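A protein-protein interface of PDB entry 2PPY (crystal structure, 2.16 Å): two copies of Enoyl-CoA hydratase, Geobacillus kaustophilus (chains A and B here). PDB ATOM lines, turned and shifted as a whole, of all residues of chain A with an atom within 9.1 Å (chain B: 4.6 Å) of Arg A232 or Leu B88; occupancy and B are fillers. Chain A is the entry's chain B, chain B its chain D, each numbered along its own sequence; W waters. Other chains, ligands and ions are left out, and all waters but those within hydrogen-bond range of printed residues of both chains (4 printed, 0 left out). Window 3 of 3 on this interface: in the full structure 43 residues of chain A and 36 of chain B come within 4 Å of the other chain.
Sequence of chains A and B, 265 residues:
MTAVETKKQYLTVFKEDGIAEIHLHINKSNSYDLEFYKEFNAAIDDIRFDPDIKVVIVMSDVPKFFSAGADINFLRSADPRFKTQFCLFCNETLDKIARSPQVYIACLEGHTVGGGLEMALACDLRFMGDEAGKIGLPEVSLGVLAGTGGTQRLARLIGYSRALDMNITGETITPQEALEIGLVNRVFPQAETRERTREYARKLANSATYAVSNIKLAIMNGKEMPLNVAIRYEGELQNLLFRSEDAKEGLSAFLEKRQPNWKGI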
ATOM      1  N   ALA A 218      -8.984 -27.095  15.262  1.00  0.00           N
ATOM      2  CA  ALA A 218     -10.344 -26.648  15.524  1.00  0.00           C
ATOM      3  C   ALA A 218     -11.216 -26.818  14.289  1.00  0.00           C
ATOM      4  O   ALA A 218     -12.334 -27.327  14.367  1.00  0.00           O
ATOM      5  CB  ALA A 218     -10.343 -25.188  15.960  1.00  0.00           C
ATOM      6  N   GLY A 222     -13.431 -30.065  14.216  1.00  0.00           N
ATOM      7  CA  GLY A 222     -14.681 -29.478  14.654  1.00  0.00           C
ATOM      8  C   GLY A 222     -15.765 -29.543  13.589  1.00  0.00           C
ATOM      9  O   GLY A 222     -16.955 -29.481  13.910  1.00  0.00           O
ATOM     10  N   MET A 225     -18.386 -32.103  14.041  1.00  0.00           N
ATOM     11  CA  MET A 225     -19.247 -31.957  15.215  1.00  0.00           C
ATOM     12  C   MET A 225     -20.437 -31.024  15.013  1.00  0.00           C
ATOM     13  O   MET A 225     -20.423 -30.168  14.127  1.00  0.00           O
ATOM     14  CB  MET A 225     -18.436 -31.393  16.391  1.00  0.00           C
ATOM     15  CG  MET A 225     -17.077 -32.031  16.642  1.00  0.00           C
ATOM     16  SD  MET A 225     -16.021 -31.036  17.974  1.00  0.00           S
ATOM     17  CE  MET A 225     -14.508 -32.235  18.085  1.00  0.00           C
ATOM     18  N   PRO A 226     -21.496 -31.190  15.834  1.00  0.00           N
ATOM     19  CA  PRO A 226     -22.679 -30.321  15.732  1.00  0.00           C
ATOM     20  C   PRO A 226     -22.142 -28.948  16.160  1.00  0.00           C
ATOM     21  O   PRO A 226     -21.282 -28.881  17.036  1.00  0.00           O
ATOM     22  CB  PRO A 226     -23.628 -30.900  16.780  1.00  0.00           C
ATOM     23  CG  PRO A 226     -23.260 -32.363  16.790  1.00  0.00           C
ATOM     24  CD  PRO A 226     -21.751 -32.321  16.743  1.00  0.00           C
ATOM     25  N   LEU A 227     -22.635 -27.871  15.557  1.00  0.00           N
ATOM     26  CA  LEU A 227     -22.154 -26.531  15.877  1.00  0.00           C
ATOM     27  C   LEU A 227     -22.107 -26.169  17.367  1.00  0.00           C
ATOM     28  O   LEU A 227     -21.079 -25.695  17.842  1.00  0.00           O
ATOM     29  CB  LEU A 227     -22.982 -25.475  15.133  1.00  0.00           C
ATOM     30  CG  LEU A 227     -22.538 -24.014  15.308  1.00  0.00           C
ATOM     31  CD1 LEU A 227     -21.156 -23.827  14.694  1.00  0.00           C
ATOM     32  CD2 LEU A 227     -23.531 -23.083  14.644  1.00  0.00           C
ATOM     33  N   ASN A 228     -23.196 -26.393  18.104  1.00  0.00           N
ATOM     34  CA  ASN A 228     -23.221 -26.034  19.525  1.00  0.00           C
ATOM     35  C   ASN A 228     -22.093 -26.638  20.366  1.00  0.00           C
ATOM     36  O   ASN A 228     -21.687 -26.033  21.358  1.00  0.00           O
ATOM     37  CB  ASN A 228     -24.571 -26.376  20.166  1.00  0.00           C
ATOM     38  CG  ASN A 228     -24.797 -25.627  21.485  1.00  0.00           C
ATOM     39  OD1 ASN A 228     -25.028 -26.232  22.531  1.00  0.00           O
ATOM     40  ND2 ASN A 228     -24.729 -24.301  21.428  1.00  0.00           N
ATOM     41  N   VAL A 229     -21.599 -27.823  20.007  1.00  0.00           N
ATOM     42  CA  VAL A 229     -20.487 -28.400  20.766  1.00  0.00           C
ATOM     43  C   VAL A 229     -19.168 -28.213  20.016  1.00  0.00           C
ATOM     44  O   VAL A 229     -18.087 -28.280  20.610  1.00  0.00           O
ATOM     45  CB  VAL A 229     -20.681 -29.897  21.098  1.00  0.00           C
ATOM     46  CG1 VAL A 229     -21.800 -30.055  22.134  1.00  0.00           C
ATOM     47  CG2 VAL A 229     -20.973 -30.689  19.839  1.00  0.00           C
ATOM     48  N   ALA A 230     -19.250 -27.961  18.713  1.00  0.00           N
ATOM     49  CA  ALA A 230     -18.038 -27.726  17.935  1.00  0.00           C
ATOM     50  C   ALA A 230     -17.377 -26.465  18.494  1.00  0.00           C
ATOM     51  O   ALA A 230     -16.150 -26.362  18.569  1.00  0.00           O
ATOM     52  CB  ALA A 230     -18.376 -27.526  16.458  1.00  0.00           C
ATOM     53  N   ILE A 231     -18.196 -25.507  18.909  1.00  0.00           N
ATOM     54  CA  ILE A 231     -17.660 -24.273  19.456  1.00  0.00           C
ATOM     55  C   ILE A 231     -17.030 -24.500  20.837  1.00  0.00           C
ATOM     56  O   ILE A 231     -16.191 -23.716  21.275  1.00  0.00           O
ATOM     57  CB  ILE A 231     -18.748 -23.186  19.498  1.00  0.00           C
ATOM     58  CG1 ILE A 231     -19.233 -22.914  18.064  1.00  0.00           C
ATOM     59  CG2 ILE A 231     -18.197 -21.909  20.130  1.00  0.00           C
ATOM     60  CD1 ILE A 231     -20.311 -21.823  17.926  1.00  0.00           C
ATOM     61  N   ARG A 232     -17.425 -25.580  21.513  1.00  0.00           N
ATOM     62  CA  ARG A 232     -16.842 -25.915  22.813  1.00  0.00           C
ATOM     63  C   ARG A 232     -15.405 -26.395  22.549  1.00  0.00           C
ATOM     64  O   ARG A 232     -14.468 -26.010  23.245  1.00  0.00           O
ATOM     65  CB  ARG A 232     -17.637 -27.037  23.495  1.00  0.00           C
ATOM     66  CG  ARG A 232     -19.116 -26.722  23.756  1.00  0.00           C
ATOM     67  CD  ARG A 232     -19.307 -25.785  24.944  1.00  0.00           C
ATOM     68  NE  ARG A 232     -18.933 -24.409  24.631  1.00  0.00           N
ATOM     69  CZ  ARG A 232     -19.644 -23.606  23.851  1.00  0.00           C
ATOM     70  NH1 ARG A 232     -20.776 -24.041  23.306  1.00  0.00           N
ATOM     71  NH2 ARG A 232     -19.224 -22.372  23.607  1.00  0.00           N
ATOM     72  N   TYR A 233     -15.251 -27.243  21.535  1.00  0.00           N
ATOM     73  CA  TYR A 233     -13.945 -27.773  21.143  1.00  0.00           C
ATOM     74  C   TYR A 233     -13.045 -26.589  20.802  1.00  0.00           C
ATOM     75  O   TYR A 233     -11.914 -26.504  21.271  1.00  0.00           O
ATOM     76  CB  TYR A 233     -14.118 -28.689  19.927  1.00  0.00           C
ATOM     77  CG  TYR A 233     -12.843 -29.242  19.311  1.00  0.00           C
ATOM     78  CD1 TYR A 233     -11.950 -30.012  20.054  1.00  0.00           C
ATOM     79  CD2 TYR A 233     -12.565 -29.042  17.963  1.00  0.00           C
ATOM     80  CE1 TYR A 233     -10.809 -30.574  19.465  1.00  0.00           C
ATOM     81  CE2 TYR A 233     -11.431 -29.601  17.363  1.00  0.00           C
ATOM     82  CZ  TYR A 233     -10.559 -30.363  18.118  1.00  0.00           C
ATOM     83  OH  TYR A 233      -9.440 -30.903  17.519  1.00  0.00           O
ATOM     84  N   GLU A 234     -13.569 -25.678  19.988  1.00  0.00           N
ATOM     85  CA  GLU A 234     -12.849 -24.475  19.592  1.00  0.00           C
ATOM     86  C   GLU A 234     -12.447 -23.707  20.854  1.00  0.00           C
ATOM     87  O   GLU A 234     -11.355 -23.146  20.935  1.00  0.00           O
ATOM     88  CB  GLU A 234     -13.757 -23.602  18.709  1.00  0.00           C
ATOM     89  CG  GLU A 234     -13.288 -22.159  18.502  1.00  0.00           C
ATOM     90  CD  GLU A 234     -14.383 -21.265  17.922  1.00  0.00           C
ATOM     91  OE1 GLU A 234     -14.636 -21.327  16.698  1.00  0.00           O
ATOM     92  OE2 GLU A 234     -15.002 -20.503  18.699  1.00  0.00           O
ATOM     93  N   GLY A 235     -13.338 -23.704  21.842  1.00  0.00           N
ATOM     94  CA  GLY A 235     -13.077 -22.999  23.084  1.00  0.00           C
ATOM     95  C   GLY A 235     -11.930 -23.549  23.912  1.00  0.00           C
ATOM     96  O   GLY A 235     -11.171 -22.776  24.496  1.00  0.00           O
ATOM     97  N   GLU A 236     -11.808 -24.874  23.982  1.00  0.00           N
ATOM     98  CA  GLU A 236     -10.733 -25.490  24.749  1.00  0.00           C
ATOM     99  C   GLU A 236      -9.397 -25.242  24.047  1.00  0.00           C
ATOM    100  O   GLU A 236      -8.380 -25.015  24.700  1.00  0.00           O
ATOM    101  CB  GLU A 236     -10.968 -26.995  24.914  1.00  0.00           C
ATOM    102  CG  GLU A 236     -12.190 -27.378  25.767  1.00  0.00           C
ATOM    103  CD  GLU A 236     -12.303 -26.588  27.067  1.00  0.00           C
ATOM    104  OE1 GLU A 236     -11.274 -26.318  27.723  1.00  0.00           O
ATOM    105  OE2 GLU A 236     -13.440 -26.244  27.444  1.00  0.00           O
ATOM    106  N   LEU A 237      -9.400 -25.293  22.718  1.00  0.00           N
ATOM    107  CA  LEU A 237      -8.183 -25.026  21.960  1.00  0.00           C
ATOM    108  C   LEU A 237      -7.779 -23.574  22.237  1.00  0.00           C
ATOM    109  O   LEU A 237      -6.595 -23.250  22.322  1.00  0.00           O
ATOM    110  CB  LEU A 237      -8.426 -25.243  20.465  1.00  0.00           C
ATOM    111  CG  LEU A 237      -8.620 -26.708  20.047  1.00  0.00           C
ATOM    112  CD1 LEU A 237      -9.165 -26.770  18.636  1.00  0.00           C
ATOM    113  CD2 LEU A 237      -7.284 -27.462  20.147  1.00  0.00           C
ATOM    114  N   GLN A 238      -8.773 -22.704  22.392  1.00  0.00           N
ATOM    115  CA  GLN A 238      -8.514 -21.299  22.688  1.00  0.00           C
ATOM    116  C   GLN A 238      -7.977 -21.155  24.125  1.00  0.00           C
ATOM    117  O   GLN A 238      -7.128 -20.303  24.389  1.00  0.00           O
ATOM    118  CB  GLN A 238      -9.793 -20.474  22.526  1.00  0.00           C
ATOM    119  CG  GLN A 238      -9.640 -18.988  22.873  1.00  0.00           C
ATOM    120  CD  GLN A 238      -9.055 -18.146  21.738  1.00  0.00           C
ATOM    121  OE1 GLN A 238      -9.660 -17.155  21.319  1.00  0.00           O
ATOM    122  NE2 GLN A 238      -7.876 -18.529  21.247  1.00  0.00           N
ATOM    123  N   ASN A 239      -8.470 -21.980  25.050  1.00  0.00           N
ATOM    124  CA  ASN A 239      -8.000 -21.928  26.438  1.00  0.00           C
ATOM    125  C   ASN A 239      -6.498 -22.227  26.496  1.00  0.00           C
ATOM    126  O   ASN A 239      -5.767 -21.643  27.296  1.00  0.00           O
ATOM    127  CB  ASN A 239      -8.750 -22.936  27.326  1.00  0.00           C
ATOM    128  CG  ASN A 239     -10.150 -22.473  27.688  1.00  0.00           C
ATOM    129  OD1 ASN A 239     -10.418 -21.272  27.752  1.00  0.00           O
ATOM    130  ND2 ASN A 239     -11.046 -23.424  27.948  1.00  0.00           N
ATOM    131  N   PHE A 242      -4.705 -19.062  25.291  1.00  0.00           N
ATOM    132  CA  PHE A 242      -4.705 -17.990  26.276  1.00  0.00           C
ATOM    133  C   PHE A 242      -3.671 -18.227  27.363  1.00  0.00           C
ATOM    134  O   PHE A 242      -3.332 -17.314  28.113  1.00  0.00           O
ATOM    135  CB  PHE A 242      -6.079 -17.854  26.934  1.00  0.00           C
ATOM    136  CG  PHE A 242      -7.103 -17.165  26.081  1.00  0.00           C
ATOM    137  CD1 PHE A 242      -6.731 -16.171  25.185  1.00  0.00           C
ATOM    138  CD2 PHE A 242      -8.452 -17.476  26.213  1.00  0.00           C
ATOM    139  CE1 PHE A 242      -7.689 -15.489  24.439  1.00  0.00           C
ATOM    140  CE2 PHE A 242      -9.418 -16.797  25.471  1.00  0.00           C
ATOM    141  CZ  PHE A 242      -9.036 -15.807  24.582  1.00  0.00           C
ATOM    142  N   THR B  84     -12.256 -17.381  29.683  1.00  0.00           N
ATOM    143  CA  THR B  84     -13.053 -18.555  29.339  1.00  0.00           C
ATOM    144  C   THR B  84     -14.535 -18.251  29.508  1.00  0.00           C
ATOM    145  O   THR B  84     -15.335 -18.518  28.610  1.00  0.00           O
ATOM    146  CB  THR B  84     -12.688 -19.765  30.239  1.00  0.00           C
ATOM    147  OG1 THR B  84     -11.316 -20.123  30.026  1.00  0.00           O
ATOM    148  CG2 THR B  84     -13.570 -20.968  29.913  1.00  0.00           C
ATOM    149  N   GLN B  85     -14.902 -17.685  30.654  1.00  0.00           N
ATOM    150  CA  GLN B  85     -16.302 -17.365  30.905  1.00  0.00           C
ATOM    151  C   GLN B  85     -16.785 -16.216  30.043  1.00  0.00           C
ATOM    152  O   GLN B  85     -17.962 -16.156  29.687  1.00  0.00           O
ATOM    153  CB  GLN B  85     -16.534 -17.044  32.380  1.00  0.00           C
ATOM    154  CG  GLN B  85     -16.361 -18.239  33.283  1.00  0.00           C
ATOM    155  CD  GLN B  85     -17.080 -19.463  32.750  1.00  0.00           C
ATOM    156  OE1 GLN B  85     -18.282 -19.422  32.480  1.00  0.00           O
ATOM    157  NE2 GLN B  85     -16.348 -20.564  32.598  1.00  0.00           N
ATOM    158  N   PHE B  86     -15.873 -15.308  29.709  1.00  0.00           N
ATOM    159  CA  PHE B  86     -16.198 -14.167  28.858  1.00  0.00           C
ATOM    160  C   PHE B  86     -16.558 -14.683  27.469  1.00  0.00           C
ATOM    161  O   PHE B  86     -17.588 -14.313  26.908  1.00  0.00           O
ATOM    162  CB  PHE B  86     -14.998 -13.213  28.759  1.00  0.00           C
ATOM    163  CG  PHE B  86     -15.145 -12.152  27.701  1.00  0.00           C
ATOM    164  CD1 PHE B  86     -16.253 -11.308  27.688  1.00  0.00           C
ATOM    165  CD2 PHE B  86     -14.163 -11.980  26.730  1.00  0.00           C
ATOM    166  CE1 PHE B  86     -16.382 -10.308  26.720  1.00  0.00           C
ATOM    167  CE2 PHE B  86     -14.281 -10.981  25.756  1.00  0.00           C
ATOM    168  CZ  PHE B  86     -15.390 -10.143  25.752  1.00  0.00           C
ATOM    169  N   CYS B  87     -15.696 -15.540  26.926  1.00  0.00           N
ATOM    170  CA  CYS B  87     -15.906 -16.120  25.601  1.00  0.00           C
ATOM    171  C   CYS B  87     -17.145 -16.997  25.584  1.00  0.00           C
ATOM    172  O   CYS B  87     -17.903 -16.988  24.616  1.00  0.00           O
ATOM    173  CB  CYS B  87     -14.691 -16.947  25.176  1.00  0.00           C
ATOM    174  SG  CYS B  87     -13.182 -15.977  24.958  1.00  0.00           S
ATOM    175  N   LEU B  88     -17.348 -17.757  26.653  1.00  0.00           N
ATOM    176  CA  LEU B  88     -18.517 -18.627  26.738  1.00  0.00           C
ATOM    177  C   LEU B  88     -19.794 -17.802  26.707  1.00  0.00           C
ATOM    178  O   LEU B  88     -20.749 -18.168  26.023  1.00  0.00           O
ATOM    179  CB  LEU B  88     -18.473 -19.477  28.018  1.00  0.00           C
ATOM    180  CG  LEU B  88     -19.697 -20.365  28.281  1.00  0.00           C
ATOM    181  CD1 LEU B  88     -19.946 -21.270  27.082  1.00  0.00           C
ATOM    182  CD2 LEU B  88     -19.479 -21.186  29.544  1.00  0.00           C
ATOM    183  N   PHE B  89     -19.815 -16.688  27.438  1.00  0.00           N
ATOM    184  CA  PHE B  89     -20.998 -15.836  27.461  1.00  0.00           C
ATOM    185  C   PHE B  89     -21.262 -15.193  26.101  1.00  0.00           C
ATOM    186  O   PHE B  89     -22.414 -15.091  25.663  1.00  0.00           O
ATOM    187  CB  PHE B  89     -20.870 -14.717  28.495  1.00  0.00           C
ATOM    188  CG  PHE B  89     -22.079 -13.817  28.543  1.00  0.00           C
ATOM    189  CD1 PHE B  89     -23.258 -14.251  29.143  1.00  0.00           C
ATOM    190  CD2 PHE B  89     -22.065 -12.569  27.926  1.00  0.00           C
ATOM    191  CE1 PHE B  89     -24.404 -13.459  29.121  1.00  0.00           C
ATOM    192  CE2 PHE B  89     -23.207 -11.771  27.901  1.00  0.00           C
ATOM    193  CZ  PHE B  89     -24.376 -12.217  28.496  1.00  0.00           C
ATOM    194  N   CYS B  90     -20.200 -14.732  25.446  1.00  0.00           N
ATOM    195  CA  CYS B  90     -20.336 -14.110  24.134  1.00  0.00           C
ATOM    196  C   CYS B  90     -20.869 -15.122  23.125  1.00  0.00           C
ATOM    197  O   CYS B  90     -21.751 -14.803  22.324  1.00  0.00           O
ATOM    198  CB  CYS B  90     -18.989 -13.564  23.652  1.00  0.00           C
ATOM    199  SG  CYS B  90     -18.359 -12.192  24.649  1.00  0.00           S
ATOM    200  N   ASN B  91     -20.346 -16.343  23.178  1.00  0.00           N
ATOM    201  CA  ASN B  91     -20.775 -17.393  22.258  1.00  0.00           C
ATOM    202  C   ASN B  91     -22.245 -17.754  22.432  1.00  0.00           C
ATOM    203  O   ASN B  91     -22.996 -17.838  21.454  1.00  0.00           O
ATOM    204  CB  ASN B  91     -19.913 -18.648  22.436  1.00  0.00           C
ATOM    205  CG  ASN B  91     -18.659 -18.618  21.585  1.00  0.00           C
ATOM    206  OD1 ASN B  91     -18.724 -18.380  20.381  1.00  0.00           O
ATOM    207  ND2 ASN B  91     -17.515 -18.871  22.201  1.00  0.00           N
ATOM    208  N   GLU B  92     -22.655 -17.970  23.676  1.00  0.00           N
ATOM    209  CA  GLU B  92     -24.037 -18.324  23.961  1.00  0.00           C
ATOM    210  C   GLU B  92     -24.979 -17.225  23.493  1.00  0.00           C
ATOM    211  O   GLU B  92     -26.094 -17.497  23.050  1.00  0.00           O
ATOM    212  CB  GLU B  92     -24.219 -18.574  25.456  1.00  0.00           C
ATOM    213  CG  GLU B  92     -23.400 -19.754  25.964  1.00  0.00           C
ATOM    214  CD  GLU B  92     -23.652 -20.048  27.422  1.00  0.00           C
ATOM    215  OE1 GLU B  92     -23.777 -19.085  28.206  1.00  0.00           O
ATOM    216  OE2 GLU B  92     -23.716 -21.243  27.787  1.00  0.00           O
HETATM  217  O   HOH W   1      -8.629 -19.464  29.427  1.00  0.00           O
HETATM  218  O   HOH W   2     -16.492 -20.773  24.541  1.00  0.00           O
HETATM  219  O   HOH W   3     -15.157 -21.118  21.639  1.00  0.00           O
HETATM  220  O   HOH W   4     -12.387 -16.302  22.438  1.00  0.00           O
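OG1 of Thr B84 lies within hydrogen-bond range of OD1 of Asn A239 (2.7 Å).
The backbone carbonyl oxygen (O) of Cys B87 is in hydrogen-bond range of the side-chain amide nitrogen (ND2) of Asn B91, at 3.1 Å. ND2 of Asn A239 sits at hydrogen-bond distance from OE1 of Glu A236 (2.9 Å). O of Asn A228 lies within hydrogen-bond range of NH1 of Arg A232 (2.9 Å).
Among the printed residues, pairs that only touch across the chains: Ile A231 with Asn B91 (3.6 Å), Arg A232 with Leu B88 (3.7 Å), Arg A232 with Asn B91 (3.96 Å) and Phe A242 with Cys B87 (3.9 Å).
Of chain B, only Leu B88 (3.7 Å) and Asn B91 (3.96 Å) come within 4 Å of Arg A232. Leu B88 touches one residue of chain A. Cys B87 touches just one residue of chain A: Phe A242. Of the printed residues of chain A, Thr B84 touches Asn A239. Printed residues of chain A within 4 Å of Asn B91: Ile A231 (3.6 Å) and Arg A232 (3.96 Å). Glu A234 touches none of the printed residues of chain B. Ala A218 touches none of the printed residues of chain B. The nearest printed residue of chain A that does not touch Asn B91 is Glu A234 (4.6 Å).
Hydrophobic or aromatic side chains of chain A that line the printed part of chain B: Ile A231 and Phe A242. Among the printed residues, no Asp or Glu carboxylate lies within 4 Å of a Lys or Arg side-chain nitrogen of the other chain.
No position is printed for both chains.
Water W4 lies within hydrogen-bond range of SG of Cys B87 and OE1 of Gln A238. Water W3 lies within hydrogen-bond range of the backbone carbonyl oxygen of Ile A231 (2.8 Å), the side-chain carboxylate of Glu A234 (3.0 Å), the backbone NH of Gly A235 (3.2 Å) and the side-chain amide nitrogen of Asn B91 (3.3 Å). Water W1 lies within hydrogen-bond range of the side-chain hydroxyl of Thr B84 (2.8 Å) and the side-chain amide oxygen of Asn A239 (3.0 Å). Water W2 bridges the side-chain amide nitrogen (ND2) of Asn B91 (3.2 Å) and the guanidinium group (NH2) of Arg A232 (3.3 Å).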
